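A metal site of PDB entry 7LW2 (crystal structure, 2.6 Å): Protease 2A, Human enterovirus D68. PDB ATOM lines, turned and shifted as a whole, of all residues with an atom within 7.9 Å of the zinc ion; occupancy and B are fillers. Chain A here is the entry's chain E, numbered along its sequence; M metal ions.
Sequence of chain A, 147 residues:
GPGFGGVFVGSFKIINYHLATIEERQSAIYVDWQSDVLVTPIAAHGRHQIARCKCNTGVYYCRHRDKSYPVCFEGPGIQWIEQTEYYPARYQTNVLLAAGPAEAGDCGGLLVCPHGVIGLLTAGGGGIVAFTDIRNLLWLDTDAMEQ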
ATOM      1  N   ALA A  51     -14.469  -0.538 -18.424  1.00  0.00           N
ATOM      2  CA  ALA A  51     -14.805  -1.900 -18.806  1.00  0.00           C
ATOM      3  C   ALA A  51     -16.214  -1.960 -19.372  1.00  0.00           C
ATOM      4  O   ALA A  51     -17.192  -1.668 -18.656  1.00  0.00           O
ATOM      5  CB  ALA A  51     -14.658  -2.838 -17.613  1.00  0.00           C
ATOM      6  N   ARG A  52     -16.335  -2.318 -20.647  1.00  0.00           N
ATOM      7  CA  ARG A  52     -17.626  -2.573 -21.280  1.00  0.00           C
ATOM      8  C   ARG A  52     -17.944  -4.064 -21.191  1.00  0.00           C
ATOM      9  O   ARG A  52     -17.926  -4.808 -22.176  1.00  0.00           O
ATOM     10  CB  ARG A  52     -17.607  -2.098 -22.735  1.00  0.00           C
ATOM     11  CG  ARG A  52     -17.490  -0.600 -22.924  1.00  0.00           C
ATOM     12  CD  ARG A  52     -17.026  -0.281 -24.343  1.00  0.00           C
ATOM     13  NE  ARG A  52     -16.585   1.104 -24.479  1.00  0.00           N
ATOM     14  CZ  ARG A  52     -17.301   2.078 -25.039  1.00  0.00           C
ATOM     15  NH1 ARG A  52     -18.523   1.844 -25.509  1.00  0.00           N
ATOM     16  NH2 ARG A  52     -16.791   3.303 -25.113  1.00  0.00           N
ATOM     17  N   CYS A  53     -18.239  -4.498 -19.969  1.00  0.00           N
ATOM     18  CA  CYS A  53     -18.435  -5.920 -19.701  1.00  0.00           C
ATOM     19  C   CYS A  53     -19.514  -6.096 -18.635  1.00  0.00           C
ATOM     20  O   CYS A  53     -20.115  -5.132 -18.154  1.00  0.00           O
ATOM     21  CB  CYS A  53     -17.141  -6.575 -19.241  1.00  0.00           C
ATOM     22  SG  CYS A  53     -16.625  -5.974 -17.631  1.00  0.00           S
ATOM     23  N   LYS A  54     -19.734  -7.364 -18.257  1.00  0.00           N
ATOM     24  CA  LYS A  54     -20.621  -7.738 -17.159  1.00  0.00           C
ATOM     25  C   LYS A  54     -19.895  -8.649 -16.177  1.00  0.00           C
ATOM     26  O   LYS A  54     -20.508  -9.519 -15.553  1.00  0.00           O
ATOM     27  CB  LYS A  54     -21.879  -8.419 -17.683  1.00  0.00           C
ATOM     28  CG  LYS A  54     -22.693  -7.564 -18.645  1.00  0.00           C
ATOM     29  CD  LYS A  54     -23.842  -8.356 -19.243  1.00  0.00           C
ATOM     30  CE  LYS A  54     -24.608  -7.548 -20.277  1.00  0.00           C
ATOM     31  NZ  LYS A  54     -25.759  -8.309 -20.826  1.00  0.00           N
ATOM     32  N   CYS A  55     -18.583  -8.465 -16.019  1.00  0.00           N
ATOM     33  CA  CYS A  55     -17.801  -9.309 -15.119  1.00  0.00           C
ATOM     34  C   CYS A  55     -18.339  -9.205 -13.692  1.00  0.00           C
ATOM     35  O   CYS A  55     -18.672  -8.120 -13.206  1.00  0.00           O
ATOM     36  CB  CYS A  55     -16.327  -8.888 -15.146  1.00  0.00           C
ATOM     37  SG  CYS A  55     -15.403  -9.438 -16.595  1.00  0.00           S
ATOM     38  N   ASN A  56     -18.415 -10.357 -13.022  1.00  0.00           N
ATOM     39  CA  ASN A  56     -18.752 -10.415 -11.601  1.00  0.00           C
ATOM     40  C   ASN A  56     -17.532 -10.673 -10.724  1.00  0.00           C
ATOM     41  O   ASN A  56     -17.684 -10.803  -9.504  1.00  0.00           O
ATOM     42  CB  ASN A  56     -19.806 -11.502 -11.362  1.00  0.00           C
ATOM     43  CG  ASN A  56     -19.410 -12.841 -11.961  1.00  0.00           C
ATOM     44  OD1 ASN A  56     -19.489 -13.051 -13.173  1.00  0.00           O
ATOM     45  ND2 ASN A  56     -18.974 -13.764 -11.106  1.00  0.00           N
ATOM     46  N   THR A  57     -16.338 -10.729 -11.307  1.00  0.00           N
ATOM     47  CA  THR A  57     -15.073 -10.841 -10.589  1.00  0.00           C
ATOM     48  C   THR A  57     -14.086  -9.788 -11.071  1.00  0.00           C
ATOM     49  O   THR A  57     -14.158  -9.296 -12.196  1.00  0.00           O
ATOM     50  CB  THR A  57     -14.408 -12.249 -10.691  1.00  0.00           C
ATOM     51  OG1 THR A  57     -14.559 -12.761 -12.029  1.00  0.00           O
ATOM     52  CG2 THR A  57     -14.819 -13.200  -9.591  1.00  0.00           C
ATOM     53  N   GLY A  58     -13.179  -9.432 -10.168  1.00  0.00           N
ATOM     54  CA  GLY A  58     -12.179  -8.431 -10.447  1.00  0.00           C
ATOM     55  C   GLY A  58     -11.116  -8.439  -9.380  1.00  0.00           C
ATOM     56  O   GLY A  58     -11.088  -9.304  -8.510  1.00  0.00           O
ATOM     57  N   PHE A  73     -17.930 -10.041  -6.666  1.00  0.00           N
ATOM     58  CA  PHE A  73     -18.817  -9.030  -6.120  1.00  0.00           C
ATOM     59  C   PHE A  73     -20.220  -9.117  -6.718  1.00  0.00           C
ATOM     60  O   PHE A  73     -20.433  -9.694  -7.783  1.00  0.00           O
ATOM     61  CB  PHE A  73     -18.249  -7.633  -6.372  1.00  0.00           C
ATOM     62  CG  PHE A  73     -17.866  -7.383  -7.805  1.00  0.00           C
ATOM     63  CD1 PHE A  73     -18.816  -7.006  -8.731  1.00  0.00           C
ATOM     64  CD2 PHE A  73     -16.554  -7.545  -8.215  1.00  0.00           C
ATOM     65  CE1 PHE A  73     -18.461  -6.780 -10.047  1.00  0.00           C
ATOM     66  CE2 PHE A  73     -16.199  -7.319  -9.531  1.00  0.00           C
ATOM     67  CZ  PHE A  73     -17.156  -6.940 -10.449  1.00  0.00           C
ATOM     68  N   VAL A 112     -10.571  -3.640 -11.161  1.00  0.00           N
ATOM     69  CA  VAL A 112     -10.350  -3.837 -12.589  1.00  0.00           C
ATOM     70  C   VAL A 112     -10.591  -5.293 -12.950  1.00  0.00           C
ATOM     71  O   VAL A 112     -10.581  -6.185 -12.108  1.00  0.00           O
ATOM     72  CB  VAL A 112      -8.927  -3.411 -13.018  1.00  0.00           C
ATOM     73  CG1 VAL A 112      -8.626  -1.991 -12.579  1.00  0.00           C
ATOM     74  CG2 VAL A 112      -7.889  -4.380 -12.468  1.00  0.00           C
ATOM     75  N   CYS A 113     -10.805  -5.512 -14.237  1.00  0.00           N
ATOM     76  CA  CYS A 113     -10.887  -6.840 -14.841  1.00  0.00           C
ATOM     77  C   CYS A 113     -10.150  -6.787 -16.165  1.00  0.00           C
ATOM     78  O   CYS A 113      -9.612  -5.733 -16.538  1.00  0.00           O
ATOM     79  CB  CYS A 113     -12.347  -7.242 -15.040  1.00  0.00           C
ATOM     80  SG  CYS A 113     -13.196  -6.241 -16.240  1.00  0.00           S
ATOM     81  N   PRO A 114     -10.075  -7.892 -16.915  1.00  0.00           N
ATOM     82  CA  PRO A 114      -9.344  -7.859 -18.188  1.00  0.00           C
ATOM     83  C   PRO A 114      -9.877  -6.829 -19.167  1.00  0.00           C
ATOM     84  O   PRO A 114      -9.147  -6.468 -20.108  1.00  0.00           O
ATOM     85  CB  PRO A 114      -9.519  -9.286 -18.727  1.00  0.00           C
ATOM     86  CG  PRO A 114      -9.771 -10.123 -17.517  1.00  0.00           C
ATOM     87  CD  PRO A 114     -10.542  -9.243 -16.571  1.00  0.00           C
ATOM     88  N   HIS A 115     -11.094  -6.339 -18.993  1.00  0.00           N
ATOM     89  CA  HIS A 115     -11.670  -5.363 -19.908  1.00  0.00           C
ATOM     90  C   HIS A 115     -11.341  -3.926 -19.543  1.00  0.00           C
ATOM     91  O   HIS A 115     -11.403  -3.062 -20.417  1.00  0.00           O
ATOM     92  CB  HIS A 115     -13.197  -5.540 -19.954  1.00  0.00           C
ATOM     93  CG  HIS A 115     -13.620  -6.932 -20.291  1.00  0.00           C
ATOM     94  ND1 HIS A 115     -14.083  -7.823 -19.335  1.00  0.00           N
ATOM     95  CD2 HIS A 115     -13.665  -7.596 -21.475  1.00  0.00           C
ATOM     96  CE1 HIS A 115     -14.386  -8.968 -19.928  1.00  0.00           C
ATOM     97  NE2 HIS A 115     -14.136  -8.854 -21.217  1.00  0.00           N
ATOM     98  N   GLY A 116     -10.984  -3.653 -18.293  1.00  0.00           N
ATOM     99  CA  GLY A 116     -10.667  -2.318 -17.854  1.00  0.00           C
ATOM    100  C   GLY A 116     -11.151  -2.092 -16.435  1.00  0.00           C
ATOM    101  O   GLY A 116     -11.344  -3.038 -15.670  1.00  0.00           O
ATOM    102  N   VAL A 117     -11.343  -0.827 -16.089  1.00  0.00           N
ATOM    103  CA  VAL A 117     -11.780  -0.450 -14.758  1.00  0.00           C
ATOM    104  C   VAL A 117     -13.290  -0.622 -14.648  1.00  0.00           C
ATOM    105  O   VAL A 117     -14.039  -0.229 -15.549  1.00  0.00           O
ATOM    106  CB  VAL A 117     -11.358   0.997 -14.430  1.00  0.00           C
ATOM    107  CG1 VAL A 117     -11.522   1.270 -12.943  1.00  0.00           C
ATOM    108  CG2 VAL A 117      -9.931   1.248 -14.872  1.00  0.00           C
ATOM    109  N   ILE A 118     -13.738  -1.200 -13.539  1.00  0.00           N
ATOM    110  CA  ILE A 118     -15.158  -1.396 -13.281  1.00  0.00           C
ATOM    111  C   ILE A 118     -15.705  -0.345 -12.324  1.00  0.00           C
ATOM    112  O   ILE A 118     -16.787   0.201 -12.561  1.00  0.00           O
ATOM    113  CB  ILE A 118     -15.405  -2.824 -12.739  1.00  0.00           C
ATOM    114  CG1 ILE A 118     -15.200  -3.863 -13.835  1.00  0.00           C
ATOM    115  CG2 ILE A 118     -16.811  -2.932 -12.171  1.00  0.00           C
ATOM    116  CD1 ILE A 118     -15.088  -5.274 -13.324  1.00  0.00           C
ATOM    117  N   ARG A 135     -19.272   1.486 -15.117  1.00  0.00           N
ATOM    118  CA  ARG A 135     -19.457   0.930 -16.453  1.00  0.00           C
ATOM    119  C   ARG A 135     -20.445   1.757 -17.257  1.00  0.00           C
ATOM    120  O   ARG A 135     -20.385   1.761 -18.491  1.00  0.00           O
ATOM    121  CB  ARG A 135     -19.925  -0.526 -16.347  1.00  0.00           C
ATOM    122  CG  ARG A 135     -18.850  -1.501 -15.887  1.00  0.00           C
ATOM    123  CD  ARG A 135     -19.260  -2.956 -16.132  1.00  0.00           C
ATOM    124  NE  ARG A 135     -19.824  -3.579 -14.934  1.00  0.00           N
ATOM    125  CZ  ARG A 135     -19.318  -4.641 -14.313  1.00  0.00           C
ATOM    126  NH1 ARG A 135     -18.212  -5.237 -14.764  1.00  0.00           N
ATOM    127  NH2 ARG A 135     -19.911  -5.126 -13.234  1.00  0.00           N
HETATM  128 ZN    ZN M   1     -14.803  -7.369 -17.462  1.00  0.00          ZN
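Of the 17 residues printed, 4 come within 4 Å of the zinc ion.
The nearest printed residue that does not touch the zinc ion is Ala 51 (4.5 Å).
ND1 of His 115 is bound to the zinc ion (2.1 Å).
The zinc ion is bound by SG of Cys 53.
The side-chain sulfur (SG) of Cys 113 binds the zinc ion.
SG of Cys 55 binds the zinc ion (2.3 Å).
The zinc ion has four donor atoms within binding distance.
The guanidinium group (NH1) of Arg 135 sits close to the side-chain sulfur (SG) of Cys 53.
The backbone carbonyl oxygen (O) of Cys 55 lies within hydrogen-bond range of the guanidinium group (NH2) of Arg 135 (3.2 Å).
The side-chain sulfur of Cys 113 sits close to the backbone carbonyl oxygen of Gly 116.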
